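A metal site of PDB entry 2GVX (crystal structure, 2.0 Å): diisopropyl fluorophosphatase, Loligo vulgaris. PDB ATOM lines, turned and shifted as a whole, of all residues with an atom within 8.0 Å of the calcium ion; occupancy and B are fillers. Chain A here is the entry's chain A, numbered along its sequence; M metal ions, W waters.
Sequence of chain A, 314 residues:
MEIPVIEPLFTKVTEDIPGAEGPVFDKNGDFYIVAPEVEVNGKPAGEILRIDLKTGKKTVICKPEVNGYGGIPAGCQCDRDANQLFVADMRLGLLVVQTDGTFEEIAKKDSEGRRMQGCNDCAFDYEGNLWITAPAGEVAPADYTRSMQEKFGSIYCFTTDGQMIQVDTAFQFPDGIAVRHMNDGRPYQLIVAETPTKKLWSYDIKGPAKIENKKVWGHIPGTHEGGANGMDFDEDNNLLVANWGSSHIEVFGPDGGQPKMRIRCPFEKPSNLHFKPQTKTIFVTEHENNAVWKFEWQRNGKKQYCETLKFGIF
The backbone NH of Leu 240 lies within hydrogen-bond range of the backbone carbonyl oxygen of Asp 232. A ring nitrogen (ND1) of His 274 lies close to the backbone carbonyl oxygen (O) of Pro 23, 3.4 Å away. O of His 274 is in hydrogen-bond range of N of Phe 283 (2.8 Å). The side-chain amide oxygen (OD1) of Asn 272 sits close to the side-chain carboxylate (OD2) of Asp 121, 3.1 Å away. The side-chain carboxylate (OE1) of Glu 21 lies close to the side-chain amide oxygen (OD1) of Asn 272 (2.6 Å).
Merely in contact with the calcium ion: Asn 272 (3.95 Å). Of the 23 residues printed, 4 come within 4 Å of the calcium ion. Along chain A the residues within 4 Å of the calcium ion span positions 232 to 274. The nearest printed residue that does not touch the calcium ion is Met 231 (4.1 Å).
OD2 of Asp 232 is bound to the calcium ion, 2.4 Å away. The backbone carbonyl oxygen (O) of Leu 273 binds the calcium ion. ND1 of His 274 binds the calcium ion, 2.6 Å away. The calcium ion is bound by water W3, 2.7 Å away. Water W2 is bound to the calcium ion (2.7 Å). Water W1 is bound to the calcium ion (2.9 Å).
Water W1 lies within hydrogen-bond range of OE1 of Gln 77 (2.8 Å) and OD1 of Asp 232 (2.8 Å). Water W2 bridges O of Met 231 and ND2 of Asn 272.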
ATOM      1  N   GLU A  21      -6.368  26.748 -12.646  1.00  0.00           N
ATOM      2  CA  GLU A  21      -5.407  26.327 -13.640  1.00  0.00           C
ATOM      3  C   GLU A  21      -4.511  27.479 -14.118  1.00  0.00           C
ATOM      4  O   GLU A  21      -4.651  28.622 -13.667  1.00  0.00           O
ATOM      5  CB  GLU A  21      -6.237  25.732 -14.788  1.00  0.00           C
ATOM      6  CG  GLU A  21      -5.541  25.373 -16.057  1.00  0.00           C
ATOM      7  CD  GLU A  21      -4.666  24.151 -15.960  1.00  0.00           C
ATOM      8  OE1 GLU A  21      -3.508  24.296 -15.543  1.00  0.00           O
ATOM      9  OE2 GLU A  21      -5.155  23.061 -16.308  1.00  0.00           O
ATOM     10  N   GLY A  22      -3.568  27.156 -14.995  1.00  0.00           N
ATOM     11  CA  GLY A  22      -2.656  28.139 -15.566  1.00  0.00           C
ATOM     12  C   GLY A  22      -1.970  29.161 -14.669  1.00  0.00           C
ATOM     13  O   GLY A  22      -2.036  30.361 -14.953  1.00  0.00           O
ATOM     14  N   PRO A  23      -1.288  28.736 -13.590  1.00  0.00           N
ATOM     15  CA  PRO A  23      -0.622  29.708 -12.712  1.00  0.00           C
ATOM     16  C   PRO A  23       0.559  30.344 -13.443  1.00  0.00           C
ATOM     17  O   PRO A  23       1.315  29.654 -14.133  1.00  0.00           O
ATOM     18  CB  PRO A  23      -0.174  28.842 -11.528  1.00  0.00           C
ATOM     19  CG  PRO A  23       0.142  27.525 -12.205  1.00  0.00           C
ATOM     20  CD  PRO A  23      -1.020  27.352 -13.166  1.00  0.00           C
ATOM     21  N   VAL A  24       0.719  31.647 -13.289  1.00  0.00           N
ATOM     22  CA  VAL A  24       1.799  32.351 -13.963  1.00  0.00           C
ATOM     23  C   VAL A  24       2.148  33.664 -13.257  1.00  0.00           C
ATOM     24  O   VAL A  24       1.320  34.237 -12.548  1.00  0.00           O
ATOM     25  CB  VAL A  24       1.403  32.655 -15.434  1.00  0.00           C
ATOM     26  CG1 VAL A  24       0.237  33.628 -15.465  1.00  0.00           C
ATOM     27  CG2 VAL A  24       2.601  33.228 -16.219  1.00  0.00           C
ATOM     28  N   PHE A  25       3.370  34.135 -13.455  1.00  0.00           N
ATOM     29  CA  PHE A  25       3.841  35.387 -12.885  1.00  0.00           C
ATOM     30  C   PHE A  25       4.213  36.321 -14.030  1.00  0.00           C
ATOM     31  O   PHE A  25       4.862  35.890 -14.984  1.00  0.00           O
ATOM     32  CB  PHE A  25       5.077  35.143 -12.017  1.00  0.00           C
ATOM     33  CG  PHE A  25       4.766  34.572 -10.661  1.00  0.00           C
ATOM     34  CD1 PHE A  25       4.478  35.414  -9.586  1.00  0.00           C
ATOM     35  CD2 PHE A  25       4.737  33.198 -10.452  1.00  0.00           C
ATOM     36  CE1 PHE A  25       4.177  34.910  -8.321  1.00  0.00           C
ATOM     37  CE2 PHE A  25       4.442  32.661  -9.187  1.00  0.00           C
ATOM     38  CZ  PHE A  25       4.160  33.532  -8.117  1.00  0.00           C
ATOM     39  N   CYS A  76      -1.371  29.596 -19.332  1.00  0.00           N
ATOM     40  CA  CYS A  76      -0.740  30.899 -19.577  1.00  0.00           C
ATOM     41  C   CYS A  76       0.782  30.912 -19.629  1.00  0.00           C
ATOM     42  O   CYS A  76       1.454  30.050 -19.066  1.00  0.00           O
ATOM     43  CB  CYS A  76      -1.164  31.900 -18.506  1.00  0.00           C
ATOM     44  SG  CYS A  76      -2.881  31.790 -18.029  1.00  0.00           S
ATOM     45  N   GLN A  77       1.296  31.946 -20.292  1.00  0.00           N
ATOM     46  CA  GLN A  77       2.721  32.213 -20.441  1.00  0.00           C
ATOM     47  C   GLN A  77       2.818  33.730 -20.479  1.00  0.00           C
ATOM     48  O   GLN A  77       1.995  34.376 -21.114  1.00  0.00           O
ATOM     49  CB  GLN A  77       3.270  31.654 -21.757  1.00  0.00           C
ATOM     50  CG  GLN A  77       3.547  30.159 -21.773  1.00  0.00           C
ATOM     51  CD  GLN A  77       4.675  29.751 -20.845  1.00  0.00           C
ATOM     52  OE1 GLN A  77       4.460  29.420 -19.686  1.00  0.00           O
ATOM     53  NE2 GLN A  77       5.901  29.781 -21.359  1.00  0.00           N
ATOM     54  N   ASP A 121      -2.654  24.568 -23.059  1.00  0.00           N
ATOM     55  CA  ASP A 121      -1.486  25.121 -22.371  1.00  0.00           C
ATOM     56  C   ASP A 121      -0.475  25.557 -23.432  1.00  0.00           C
ATOM     57  O   ASP A 121      -0.614  25.245 -24.607  1.00  0.00           O
ATOM     58  CB  ASP A 121      -0.875  24.078 -21.421  1.00  0.00           C
ATOM     59  CG  ASP A 121      -0.188  24.717 -20.211  1.00  0.00           C
ATOM     60  OD1 ASP A 121       0.123  25.916 -20.256  1.00  0.00           O
ATOM     61  OD2 ASP A 121       0.050  24.000 -19.208  1.00  0.00           O
ATOM     62  N   CYS A 122       0.534  26.312 -23.020  1.00  0.00           N
ATOM     63  CA  CYS A 122       1.556  26.775 -23.960  1.00  0.00           C
ATOM     64  C   CYS A 122       2.875  26.986 -23.246  1.00  0.00           C
ATOM     65  O   CYS A 122       2.922  27.023 -22.014  1.00  0.00           O
ATOM     66  CB  CYS A 122       1.116  28.086 -24.625  1.00  0.00           C
ATOM     67  SG  CYS A 122       0.622  29.409 -23.489  1.00  0.00           S
ATOM     68  N   ALA A 123       3.945  27.111 -24.034  1.00  0.00           N
ATOM     69  CA  ALA A 123       5.291  27.298 -23.486  1.00  0.00           C
ATOM     70  C   ALA A 123       6.202  28.006 -24.488  1.00  0.00           C
ATOM     71  O   ALA A 123       6.342  27.573 -25.634  1.00  0.00           O
ATOM     72  CB  ALA A 123       5.878  25.953 -23.107  1.00  0.00           C
ATOM     73  N   ILE A 177       2.882  21.115 -21.679  1.00  0.00           N
ATOM     74  CA  ILE A 177       3.904  21.236 -22.691  1.00  0.00           C
ATOM     75  C   ILE A 177       5.078  22.037 -22.130  1.00  0.00           C
ATOM     76  O   ILE A 177       4.904  22.898 -21.275  1.00  0.00           O
ATOM     77  CB  ILE A 177       3.319  21.919 -23.952  1.00  0.00           C
ATOM     78  CG1 ILE A 177       4.355  21.972 -25.072  1.00  0.00           C
ATOM     79  CG2 ILE A 177       2.817  23.313 -23.600  1.00  0.00           C
ATOM     80  CD1 ILE A 177       3.751  22.340 -26.435  1.00  0.00           C
ATOM     81  N   GLY A 230      -0.272  19.796 -16.209  1.00  0.00           N
ATOM     82  CA  GLY A 230       0.685  20.874 -16.435  1.00  0.00           C
ATOM     83  C   GLY A 230       2.113  20.488 -16.078  1.00  0.00           C
ATOM     84  O   GLY A 230       2.325  19.538 -15.325  1.00  0.00           O
ATOM     85  N   MET A 231       3.093  21.236 -16.604  1.00  0.00           N
ATOM     86  CA  MET A 231       4.508  20.933 -16.350  1.00  0.00           C
ATOM     87  C   MET A 231       5.473  22.124 -16.460  1.00  0.00           C
ATOM     88  O   MET A 231       5.155  23.150 -17.066  1.00  0.00           O
ATOM     89  CB  MET A 231       4.967  19.850 -17.324  1.00  0.00           C
ATOM     90  CG  MET A 231       4.894  20.279 -18.785  1.00  0.00           C
ATOM     91  SD  MET A 231       5.564  19.083 -19.977  1.00  0.00           S
ATOM     92  CE  MET A 231       4.384  17.776 -19.796  1.00  0.00           C
ATOM     93  N   ASP A 232       6.662  21.964 -15.878  1.00  0.00           N
ATOM     94  CA  ASP A 232       7.721  22.983 -15.922  1.00  0.00           C
ATOM     95  C   ASP A 232       9.054  22.386 -15.522  1.00  0.00           C
ATOM     96  O   ASP A 232       9.109  21.431 -14.749  1.00  0.00           O
ATOM     97  CB  ASP A 232       7.439  24.138 -14.957  1.00  0.00           C
ATOM     98  CG  ASP A 232       6.689  25.289 -15.591  1.00  0.00           C
ATOM     99  OD1 ASP A 232       6.815  25.541 -16.812  1.00  0.00           O
ATOM    100  OD2 ASP A 232       5.972  25.963 -14.841  1.00  0.00           O
ATOM    101  N   PHE A 233      10.139  22.974 -16.025  1.00  0.00           N
ATOM    102  CA  PHE A 233      11.491  22.529 -15.707  1.00  0.00           C
ATOM    103  C   PHE A 233      12.083  23.323 -14.556  1.00  0.00           C
ATOM    104  O   PHE A 233      11.697  24.483 -14.333  1.00  0.00           O
ATOM    105  CB  PHE A 233      12.433  22.754 -16.893  1.00  0.00           C
ATOM    106  CG  PHE A 233      12.336  21.714 -17.969  1.00  0.00           C
ATOM    107  CD1 PHE A 233      12.861  20.443 -17.757  1.00  0.00           C
ATOM    108  CD2 PHE A 233      11.784  22.018 -19.203  1.00  0.00           C
ATOM    109  CE1 PHE A 233      12.822  19.477 -18.764  1.00  0.00           C
ATOM    110  CE2 PHE A 233      11.752  21.060 -20.221  1.00  0.00           C
ATOM    111  CZ  PHE A 233      12.263  19.792 -20.004  1.00  0.00           C
ATOM    112  N   LEU A 240       9.149  18.716 -13.834  1.00  0.00           N
ATOM    113  CA  LEU A 240       8.121  18.440 -12.831  1.00  0.00           C
ATOM    114  C   LEU A 240       6.761  18.451 -13.525  1.00  0.00           C
ATOM    115  O   LEU A 240       6.376  19.423 -14.170  1.00  0.00           O
ATOM    116  CB  LEU A 240       8.155  19.482 -11.694  1.00  0.00           C
ATOM    117  CG  LEU A 240       9.329  19.373 -10.707  1.00  0.00           C
ATOM    118  CD1 LEU A 240      10.596  19.987 -11.307  1.00  0.00           C
ATOM    119  CD2 LEU A 240       8.979  20.066  -9.410  1.00  0.00           C
ATOM    120  N   ASN A 272      -1.773  22.058 -12.421  1.00  0.00           N
ATOM    121  CA  ASN A 272      -0.684  22.796 -13.045  1.00  0.00           C
ATOM    122  C   ASN A 272       0.216  23.375 -11.975  1.00  0.00           C
ATOM    123  O   ASN A 272      -0.138  23.396 -10.797  1.00  0.00           O
ATOM    124  CB  ASN A 272      -1.263  23.894 -13.945  1.00  0.00           C
ATOM    125  CG  ASN A 272      -0.478  24.090 -15.225  1.00  0.00           C
ATOM    126  OD1 ASN A 272      -1.049  24.384 -16.285  1.00  0.00           O
ATOM    127  ND2 ASN A 272       0.838  23.927 -15.141  1.00  0.00           N
ATOM    128  N   LEU A 273       1.387  23.855 -12.371  1.00  0.00           N
ATOM    129  CA  LEU A 273       2.337  24.423 -11.414  1.00  0.00           C
ATOM    130  C   LEU A 273       3.162  25.494 -12.099  1.00  0.00           C
ATOM    131  O   LEU A 273       3.117  25.623 -13.296  1.00  0.00           O
ATOM    132  CB  LEU A 273       3.238  23.313 -10.864  1.00  0.00           C
ATOM    133  CG  LEU A 273       3.950  22.374 -11.846  1.00  0.00           C
ATOM    134  CD1 LEU A 273       5.087  23.094 -12.542  1.00  0.00           C
ATOM    135  CD2 LEU A 273       4.509  21.180 -11.085  1.00  0.00           C
ATOM    136  N   HIS A 274       3.921  26.257 -11.325  1.00  0.00           N
ATOM    137  CA  HIS A 274       4.745  27.315 -11.895  1.00  0.00           C
ATOM    138  C   HIS A 274       5.648  27.833 -10.789  1.00  0.00           C
ATOM    139  O   HIS A 274       5.193  28.002  -9.661  1.00  0.00           O
ATOM    140  CB  HIS A 274       3.858  28.449 -12.399  1.00  0.00           C
ATOM    141  CG  HIS A 274       4.513  29.316 -13.437  1.00  0.00           C
ATOM    142  ND1 HIS A 274       4.624  28.940 -14.752  1.00  0.00           N
ATOM    143  CD2 HIS A 274       5.062  30.549 -13.356  1.00  0.00           C
ATOM    144  CE1 HIS A 274       5.209  29.902 -15.444  1.00  0.00           C
ATOM    145  NE2 HIS A 274       5.491  30.889 -14.616  1.00  0.00           N
ATOM    146  N   PHE A 275       6.902  28.099 -11.117  1.00  0.00           N
ATOM    147  CA  PHE A 275       7.842  28.628 -10.136  1.00  0.00           C
ATOM    148  C   PHE A 275       7.682  30.128  -9.989  1.00  0.00           C
ATOM    149  O   PHE A 275       7.320  30.810 -10.946  1.00  0.00           O
ATOM    150  CB  PHE A 275       9.294  28.378 -10.564  1.00  0.00           C
ATOM    151  CG  PHE A 275       9.762  26.957 -10.377  1.00  0.00           C
ATOM    152  CD1 PHE A 275       9.504  25.997 -11.354  1.00  0.00           C
ATOM    153  CD2 PHE A 275      10.472  26.596  -9.245  1.00  0.00           C
ATOM    154  CE1 PHE A 275       9.974  24.687 -11.202  1.00  0.00           C
ATOM    155  CE2 PHE A 275      10.940  25.292  -9.080  1.00  0.00           C
ATOM    156  CZ  PHE A 275      10.691  24.337 -10.058  1.00  0.00           C
ATOM    157  N   ILE A 282       7.161  26.744  -5.668  1.00  0.00           N
ATOM    158  CA  ILE A 282       6.312  26.296  -6.759  1.00  0.00           C
ATOM    159  C   ILE A 282       4.852  26.470  -6.360  1.00  0.00           C
ATOM    160  O   ILE A 282       4.409  25.986  -5.318  1.00  0.00           O
ATOM    161  CB  ILE A 282       6.554  24.795  -7.089  1.00  0.00           C
ATOM    162  CG1 ILE A 282       7.977  24.613  -7.630  1.00  0.00           C
ATOM    163  CG2 ILE A 282       5.521  24.302  -8.099  1.00  0.00           C
ATOM    164  CD1 ILE A 282       8.312  23.181  -8.011  1.00  0.00           C
ATOM    165  N   PHE A 283       4.097  27.177  -7.201  1.00  0.00           N
ATOM    166  CA  PHE A 283       2.680  27.392  -6.932  1.00  0.00           C
ATOM    167  C   PHE A 283       1.913  26.353  -7.715  1.00  0.00           C
ATOM    168  O   PHE A 283       2.141  26.183  -8.920  1.00  0.00           O
ATOM    169  CB  PHE A 283       2.261  28.805  -7.328  1.00  0.00           C
ATOM    170  CG  PHE A 283       2.795  29.857  -6.402  1.00  0.00           C
ATOM    171  CD1 PHE A 283       4.162  30.093  -6.318  1.00  0.00           C
ATOM    172  CD2 PHE A 283       1.937  30.571  -5.580  1.00  0.00           C
ATOM    173  CE1 PHE A 283       4.676  31.029  -5.429  1.00  0.00           C
ATOM    174  CE2 PHE A 283       2.434  31.519  -4.683  1.00  0.00           C
ATOM    175  CZ  PHE A 283       3.809  31.739  -4.606  1.00  0.00           C
ATOM    176  N   GLN A 304      12.117  31.615 -16.981  1.00  0.00           N
ATOM    177  CA  GLN A 304      11.126  31.669 -18.044  1.00  0.00           C
ATOM    178  C   GLN A 304      11.541  32.714 -19.084  1.00  0.00           C
ATOM    179  O   GLN A 304      12.354  33.604 -18.806  1.00  0.00           O
ATOM    180  CB  GLN A 304       9.735  32.003 -17.481  1.00  0.00           C
ATOM    181  CG  GLN A 304       9.071  30.848 -16.714  1.00  0.00           C
ATOM    182  CD  GLN A 304       8.179  29.990 -17.595  1.00  0.00           C
ATOM    183  OE1 GLN A 304       8.175  28.754 -17.484  1.00  0.00           O
ATOM    184  NE2 GLN A 304       7.399  30.634 -18.457  1.00  0.00           N
HETATM  185 CA    CA M   1       3.712  26.620 -15.462  1.00  0.00          CA
HETATM  186  O   HOH W   1       4.993  27.314 -17.955  1.00  0.00           O
HETATM  187  O   HOH W   2       3.026  24.148 -16.448  1.00  0.00           O
HETATM  188  O   HOH W   3       1.202  27.537 -15.319  1.00  0.00           O
